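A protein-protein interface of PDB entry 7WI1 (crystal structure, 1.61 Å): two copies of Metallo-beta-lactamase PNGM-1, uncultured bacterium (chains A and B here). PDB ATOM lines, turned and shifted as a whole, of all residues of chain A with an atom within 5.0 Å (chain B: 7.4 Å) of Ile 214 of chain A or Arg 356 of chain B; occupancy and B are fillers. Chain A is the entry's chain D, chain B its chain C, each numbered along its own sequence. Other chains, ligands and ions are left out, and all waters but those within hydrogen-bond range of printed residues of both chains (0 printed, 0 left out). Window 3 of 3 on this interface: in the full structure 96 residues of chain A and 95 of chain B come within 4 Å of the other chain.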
ATOM      1  N   ILE A 186      19.047  -6.606  -0.176  1.00  0.00           N
ATOM      2  CA  ILE A 186      20.062  -5.828   0.566  1.00  0.00           C
ATOM      3  C   ILE A 186      20.357  -4.617  -0.310  1.00  0.00           C
ATOM      4  O   ILE A 186      21.203  -4.729  -1.221  1.00  0.00           O
ATOM      5  CB  ILE A 186      21.340  -6.651   0.843  1.00  0.00           C
ATOM      6  CG1 ILE A 186      20.956  -7.998   1.464  1.00  0.00           C
ATOM      7  CG2 ILE A 186      22.299  -5.845   1.679  1.00  0.00           C
ATOM      8  CD1 ILE A 186      22.146  -8.889   1.756  1.00  0.00           C
ATOM      9  N   ALA A 211      22.262  -5.992  -3.535  1.00  0.00           N
ATOM     10  CA  ALA A 211      23.614  -6.554  -3.516  1.00  0.00           C
ATOM     11  C   ALA A 211      23.427  -8.062  -3.394  1.00  0.00           C
ATOM     12  O   ALA A 211      22.380  -8.541  -3.015  1.00  0.00           O
ATOM     13  CB  ALA A 211      24.405  -5.987  -2.377  1.00  0.00           C
ATOM     14  N   PRO A 212      24.433  -8.885  -3.747  1.00  0.00           N
ATOM     15  CA  PRO A 212      24.174 -10.321  -3.804  1.00  0.00           C
ATOM     16  C   PRO A 212      23.731 -10.885  -2.448  1.00  0.00           C
ATOM     17  O   PRO A 212      24.330 -10.544  -1.452  1.00  0.00           O
ATOM     18  CB  PRO A 212      25.528 -10.855  -4.271  1.00  0.00           C
ATOM     19  CG  PRO A 212      26.147  -9.702  -5.037  1.00  0.00           C
ATOM     20  CD  PRO A 212      25.760  -8.480  -4.225  1.00  0.00           C
ATOM     21  N   ASN A 213      22.712 -11.714  -2.478  1.00  0.00           N
ATOM     22  CA  ASN A 213      22.115 -12.204  -1.216  1.00  0.00           C
ATOM     23  C   ASN A 213      21.763 -13.687  -1.342  1.00  0.00           C
ATOM     24  O   ASN A 213      21.691 -14.233  -2.478  1.00  0.00           O
ATOM     25  CB  ASN A 213      20.925 -11.323  -0.810  1.00  0.00           C
ATOM     26  CG  ASN A 213      19.717 -11.557  -1.673  1.00  0.00           C
ATOM     27  OD1 ASN A 213      19.127 -12.618  -1.679  1.00  0.00           O
ATOM     28  ND2 ASN A 213      19.295 -10.522  -2.385  1.00  0.00           N
ATOM     29  N   ILE A 214      21.578 -14.335  -0.186  1.00  0.00           N
ATOM     30  CA  ILE A 214      21.428 -15.821  -0.120  1.00  0.00           C
ATOM     31  C   ILE A 214      20.012 -16.230  -0.488  1.00  0.00           C
ATOM     32  O   ILE A 214      19.781 -17.414  -0.766  1.00  0.00           O
ATOM     33  CB  ILE A 214      21.848 -16.372   1.261  1.00  0.00           C
ATOM     34  CG1 ILE A 214      20.883 -15.836   2.335  1.00  0.00           C
ATOM     35  CG2 ILE A 214      23.308 -16.056   1.538  1.00  0.00           C
ATOM     36  CD1 ILE A 214      21.128 -16.381   3.733  1.00  0.00           C
ATOM     37  N   TRP A 215      19.073 -15.281  -0.529  1.00  0.00           N
ATOM     38  CA  TRP A 215      17.642 -15.544  -0.713  1.00  0.00           C
ATOM     39  C   TRP A 215      17.313 -15.758  -2.191  1.00  0.00           C
ATOM     40  O   TRP A 215      16.685 -16.744  -2.507  1.00  0.00           O
ATOM     41  CB  TRP A 215      16.765 -14.465  -0.059  1.00  0.00           C
ATOM     42  CG  TRP A 215      16.996 -14.356   1.413  1.00  0.00           C
ATOM     43  CD1 TRP A 215      16.817 -15.332   2.357  1.00  0.00           C
ATOM     44  CD2 TRP A 215      17.499 -13.207   2.096  1.00  0.00           C
ATOM     45  NE1 TRP A 215      17.207 -14.863   3.590  1.00  0.00           N
ATOM     46  CE2 TRP A 215      17.640 -13.561   3.456  1.00  0.00           C
ATOM     47  CE3 TRP A 215      17.891 -11.924   1.671  1.00  0.00           C
ATOM     48  CZ2 TRP A 215      18.124 -12.659   4.390  1.00  0.00           C
ATOM     49  CZ3 TRP A 215      18.363 -11.038   2.608  1.00  0.00           C
ATOM     50  CH2 TRP A 215      18.457 -11.395   3.947  1.00  0.00           C
ATOM     51  N   TYR A 216      17.702 -14.837  -3.061  1.00  0.00           N
ATOM     52  CA  TYR A 216      17.323 -14.879  -4.492  1.00  0.00           C
ATOM     53  C   TYR A 216      17.806 -16.197  -5.124  1.00  0.00           C
ATOM     54  O   TYR A 216      16.990 -16.812  -5.781  1.00  0.00           O
ATOM     55  CB  TYR A 216      17.900 -13.664  -5.231  1.00  0.00           C
ATOM     56  CG  TYR A 216      17.456 -13.546  -6.662  1.00  0.00           C
ATOM     57  CD1 TYR A 216      17.977 -14.373  -7.656  1.00  0.00           C
ATOM     58  CD2 TYR A 216      16.551 -12.583  -7.048  1.00  0.00           C
ATOM     59  CE1 TYR A 216      17.597 -14.248  -8.981  1.00  0.00           C
ATOM     60  CE2 TYR A 216      16.131 -12.480  -8.364  1.00  0.00           C
ATOM     61  CZ  TYR A 216      16.647 -13.311  -9.339  1.00  0.00           C
ATOM     62  OH  TYR A 216      16.222 -13.143 -10.628  1.00  0.00           O
ATOM     63  N   PRO A 217      19.067 -16.674  -4.914  1.00  0.00           N
ATOM     64  CA  PRO A 217      19.551 -17.911  -5.555  1.00  0.00           C
ATOM     65  C   PRO A 217      18.691 -19.123  -5.160  1.00  0.00           C
ATOM     66  O   PRO A 217      18.431 -19.968  -5.984  1.00  0.00           O
ATOM     67  CB  PRO A 217      21.001 -18.070  -5.064  1.00  0.00           C
ATOM     68  CG  PRO A 217      21.415 -16.670  -4.655  1.00  0.00           C
ATOM     69  CD  PRO A 217      20.127 -16.070  -4.105  1.00  0.00           C
ATOM     70  N   GLU A 218      18.180 -19.135  -3.929  1.00  0.00           N
ATOM     71  CA  GLU A 218      17.291 -20.229  -3.442  1.00  0.00           C
ATOM     72  C   GLU A 218      15.881 -20.064  -4.005  1.00  0.00           C
ATOM     73  O   GLU A 218      15.339 -20.992  -4.617  1.00  0.00           O
ATOM     74  CB  GLU A 218      17.312 -20.225  -1.906  1.00  0.00           C
ATOM     75  CG  GLU A 218      16.539 -21.363  -1.279  1.00  0.00           C
ATOM     76  CD  GLU A 218      16.976 -22.759  -1.716  1.00  0.00           C
ATOM     77  OE1 GLU A 218      18.196 -22.983  -1.965  1.00  0.00           O
ATOM     78  OE2 GLU A 218      16.086 -23.623  -1.823  1.00  0.00           O
ATOM     79  N   ASP A 254      30.123  -4.140  -2.676  1.00  0.00           N
ATOM     80  CA  ASP A 254      29.314  -3.908  -1.445  1.00  0.00           C
ATOM     81  C   ASP A 254      27.913  -3.397  -1.792  1.00  0.00           C
ATOM     82  O   ASP A 254      26.950  -3.877  -1.198  1.00  0.00           O
ATOM     83  CB  ASP A 254      29.990  -2.916  -0.501  1.00  0.00           C
ATOM     84  CG  ASP A 254      31.380  -3.326  -0.041  1.00  0.00           C
ATOM     85  OD1 ASP A 254      31.665  -4.541  -0.066  1.00  0.00           O
ATOM     86  OD2 ASP A 254      32.185  -2.414   0.309  1.00  0.00           O
ATOM     87  N   TYR B 348      19.799  -0.046   7.770  1.00  0.00           N
ATOM     88  CA  TYR B 348      19.784  -1.533   7.755  1.00  0.00           C
ATOM     89  C   TYR B 348      19.631  -2.077   9.174  1.00  0.00           C
ATOM     90  O   TYR B 348      20.193  -1.516  10.127  1.00  0.00           O
ATOM     91  CB  TYR B 348      21.084  -2.132   7.233  1.00  0.00           C
ATOM     92  CG  TYR B 348      21.383  -1.912   5.783  1.00  0.00           C
ATOM     93  CD1 TYR B 348      20.642  -2.563   4.834  1.00  0.00           C
ATOM     94  CD2 TYR B 348      22.464  -1.150   5.400  1.00  0.00           C
ATOM     95  CE1 TYR B 348      20.940  -2.448   3.487  1.00  0.00           C
ATOM     96  CE2 TYR B 348      22.796  -1.038   4.050  1.00  0.00           C
ATOM     97  CZ  TYR B 348      22.038  -1.703   3.108  1.00  0.00           C
ATOM     98  OH  TYR B 348      22.317  -1.629   1.771  1.00  0.00           O
ATOM     99  N   TYR B 351      19.543  -8.388  10.549  1.00  0.00           N
ATOM    100  CA  TYR B 351      18.728  -9.423   9.895  1.00  0.00           C
ATOM    101  C   TYR B 351      18.912  -9.336   8.378  1.00  0.00           C
ATOM    102  O   TYR B 351      19.197 -10.350   7.756  1.00  0.00           O
ATOM    103  CB  TYR B 351      17.258  -9.268  10.238  1.00  0.00           C
ATOM    104  CG  TYR B 351      16.309 -10.199   9.530  1.00  0.00           C
ATOM    105  CD1 TYR B 351      16.051 -11.480  10.001  1.00  0.00           C
ATOM    106  CD2 TYR B 351      15.670  -9.835   8.356  1.00  0.00           C
ATOM    107  CE1 TYR B 351      15.131 -12.323   9.395  1.00  0.00           C
ATOM    108  CE2 TYR B 351      14.786 -10.673   7.711  1.00  0.00           C
ATOM    109  CZ  TYR B 351      14.521 -11.938   8.206  1.00  0.00           C
ATOM    110  OH  TYR B 351      13.629 -12.743   7.558  1.00  0.00           O
ATOM    111  N   ILE B 352      18.858  -8.125   7.824  1.00  0.00           N
ATOM    112  CA  ILE B 352      19.068  -7.972   6.355  1.00  0.00           C
ATOM    113  C   ILE B 352      20.556  -8.142   6.017  1.00  0.00           C
ATOM    114  O   ILE B 352      20.849  -8.872   5.023  1.00  0.00           O
ATOM    115  CB  ILE B 352      18.504  -6.605   5.899  1.00  0.00           C
ATOM    116  CG1 ILE B 352      16.979  -6.539   5.999  1.00  0.00           C
ATOM    117  CG2 ILE B 352      19.006  -6.293   4.478  1.00  0.00           C
ATOM    118  CD1 ILE B 352      16.215  -7.649   5.274  1.00  0.00           C
ATOM    119  N   LEU B 353      21.477  -7.493   6.724  1.00  0.00           N
ATOM    120  CA  LEU B 353      22.926  -7.607   6.428  1.00  0.00           C
ATOM    121  C   LEU B 353      23.393  -9.061   6.542  1.00  0.00           C
ATOM    122  O   LEU B 353      24.342  -9.438   5.852  1.00  0.00           O
ATOM    123  CB  LEU B 353      23.731  -6.678   7.331  1.00  0.00           C
ATOM    124  CG  LEU B 353      23.454  -5.199   7.089  1.00  0.00           C
ATOM    125  CD1 LEU B 353      24.304  -4.309   7.995  1.00  0.00           C
ATOM    126  CD2 LEU B 353      23.670  -4.844   5.635  1.00  0.00           C
ATOM    127  N   ASP B 354      22.745  -9.869   7.359  1.00  0.00           N
ATOM    128  CA  ASP B 354      23.186 -11.289   7.508  1.00  0.00           C
ATOM    129  C   ASP B 354      22.915 -12.103   6.237  1.00  0.00           C
ATOM    130  O   ASP B 354      23.332 -13.285   6.183  1.00  0.00           O
ATOM    131  CB  ASP B 354      22.479 -11.959   8.683  1.00  0.00           C
ATOM    132  CG  ASP B 354      23.105 -11.652  10.021  1.00  0.00           C
ATOM    133  OD1 ASP B 354      24.195 -11.071  10.033  1.00  0.00           O
ATOM    134  OD2 ASP B 354      22.461 -11.979  11.046  1.00  0.00           O
ATOM    135  N   GLY B 355      22.176 -11.562   5.260  1.00  0.00           N
ATOM    136  CA  GLY B 355      21.824 -12.291   4.044  1.00  0.00           C
ATOM    137  C   GLY B 355      22.861 -12.149   2.934  1.00  0.00           C
ATOM    138  O   GLY B 355      22.574 -12.673   1.887  1.00  0.00           O
ATOM    139  N   ARG B 356      24.002 -11.483   3.120  1.00  0.00           N
ATOM    140  CA  ARG B 356      24.976 -11.225   2.009  1.00  0.00           C
ATOM    141  C   ARG B 356      25.471 -12.575   1.470  1.00  0.00           C
ATOM    142  O   ARG B 356      25.727 -13.505   2.283  1.00  0.00           O
ATOM    143  CB  ARG B 356      26.128 -10.320   2.449  1.00  0.00           C
ATOM    144  CG  ARG B 356      25.748  -8.865   2.724  1.00  0.00           C
ATOM    145  CD  ARG B 356      26.980  -7.981   2.756  1.00  0.00           C
ATOM    146  NE  ARG B 356      26.663  -6.573   3.013  1.00  0.00           N
ATOM    147  CZ  ARG B 356      26.453  -5.644   2.066  1.00  0.00           C
ATOM    148  NH1 ARG B 356      26.544  -5.962   0.786  1.00  0.00           N
ATOM    149  NH2 ARG B 356      26.162  -4.395   2.403  1.00  0.00           N
ATOM    150  N   LEU B 357      25.553 -12.696   0.140  1.00  0.00           N
ATOM    151  CA  LEU B 357      26.038 -13.920  -0.552  1.00  0.00           C
ATOM    152  C   LEU B 357      27.548 -13.782  -0.755  1.00  0.00           C
ATOM    153  O   LEU B 357      28.016 -12.704  -1.161  1.00  0.00           O
ATOM    154  CB  LEU B 357      25.306 -14.058  -1.885  1.00  0.00           C
ATOM    155  CG  LEU B 357      25.741 -15.226  -2.770  1.00  0.00           C
ATOM    156  CD1 LEU B 357      25.327 -16.526  -2.124  1.00  0.00           C
ATOM    157  CD2 LEU B 357      25.098 -15.116  -4.146  1.00  0.00           C
ATOM    158  N   ASN B 358      28.325 -14.838  -0.455  1.00  0.00           N
ATOM    159  CA  ASN B 358      29.780 -14.831  -0.729  1.00  0.00           C
ATOM    160  C   ASN B 358      30.000 -14.923  -2.243  1.00  0.00           C
ATOM    161  O   ASN B 358      29.536 -15.925  -2.827  1.00  0.00           O
ATOM    162  CB  ASN B 358      30.503 -15.978  -0.018  1.00  0.00           C
ATOM    163  CG  ASN B 358      32.001 -15.754  -0.023  1.00  0.00           C
ATOM    164  OD1 ASN B 358      32.631 -15.718  -1.078  1.00  0.00           O
ATOM    165  ND2 ASN B 358      32.591 -15.585   1.144  1.00  0.00           N
ATOM    166  N   VAL B 359      30.597 -13.879  -2.836  1.00  0.00           N
ATOM    167  CA  VAL B 359      30.891 -13.796  -4.302  1.00  0.00           C
ATOM    168  C   VAL B 359      32.387 -13.579  -4.532  1.00  0.00           C
ATOM    169  O   VAL B 359      32.740 -13.135  -5.641  1.00  0.00           O
ATOM    170  CB  VAL B 359      30.037 -12.691  -4.971  1.00  0.00           C
ATOM    171  CG1 VAL B 359      28.598 -13.123  -5.007  1.00  0.00           C
ATOM    172  CG2 VAL B 359      30.181 -11.327  -4.282  1.00  0.00           C
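The backbone NH (N) of Ile 214 of chain A lies within hydrogen-bond range of the backbone carbonyl oxygen (O) of Gly 355 of chain B. NH1 of Arg 356 of chain B is in hydrogen-bond range of O of Asp 254 of chain A (2.9 Å). N of Leu 357 of chain B is in hydrogen-bond range of O of Pro 212 of chain A, 2.9 Å away.
O of Ile 186 of chain A sits at hydrogen-bond distance from N of Ala 211 of chain A (2.8 Å). The side-chain amide oxygen (OD1) of Asn 213 of chain A lies within hydrogen-bond range of the backbone NH (N) of Trp 215 of chain A (2.9 Å). OD1 of Asn 213 of chain A sits at hydrogen-bond distance from N of Tyr 216 of chain A (3.0 Å).
Among the printed residues, merely in contact across the chains: Ile 186 of chain A with Ile 352 of chain B (3.5 Å), Ile 186 of chain A with Gly 355 of chain B (3.5 Å), Ile 186 of chain A with Arg 356 of chain B (3.5 Å), Ala 211 of chain A with Arg 356 of chain B (3.8 Å), Pro 212 of chain A with Arg 356 of chain B (3.6 Å), Pro 212 of chain A with Val 359 of chain B (3.9 Å), Asn 213 of chain A with Gly 355 of chain B (3.2 Å), Asn 213 of chain A with Leu 357 of chain B (3.5 Å), Ile 214 of chain A with Arg 356 of chain B (3.6 Å), Trp 215 of chain A with Ile 352 of chain B (3.6 Å) and Trp 215 of chain A with Gly 355 of chain B (3.5 Å).
Of chain B, only Gly 355 and Arg 356 come within 4 Å of Ile 214 of chain A. Arg 356 of chain B touches just these residues of chain A: Ile 186 (3.5 Å), Ala 211 (3.8 Å), Pro 212 (3.6 Å), Ile 214 (3.6 Å) and Asp 254 (2.9 Å). Printed residues of chain B within 4 Å of Trp 215 of chain A: Ile 352 and Gly 355. Of the printed residues of chain B, Asn 213 of chain A touches Gly 355 (3.2 Å) and Leu 357 (3.5 Å). The nearest residue of chain B that does not touch Ile 214 of chain A is Leu 357 of chain B (4.05 Å). The nearest residue of chain A that does not touch Arg 356 of chain B is Asn 213 of chain A (4.3 Å). The nearest printed residue of chain B that does not touch Asp 254 of chain A is Tyr 348 of chain B (5.9 Å).
Of the 10 printed residues of chain B, 5 touch a printed residue of chain A. Printed residues of chain B that touch a printed residue of chain A: Ile 352, Gly 355, Arg 356, Leu 357 and Val 359. Hydrophobic or aromatic side chains of chain B that line the printed part of chain A: Ile 352, Leu 357 and Val 359. Along chain B the printed residues that touch a printed residue of chain A span positions 352 to 359. Hydrophobic or aromatic side chains of chain A that line the printed part of chain B: Ile 186, Ala 211, Pro 212, Ile 214 and Trp 215. Among the printed residues, 14 pairs touch across the chains. Among the printed residues, no Asp or Glu carboxylate lies within 4 Å of a Lys or Arg side-chain nitrogen of the other chain.
No position is printed for both chains.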
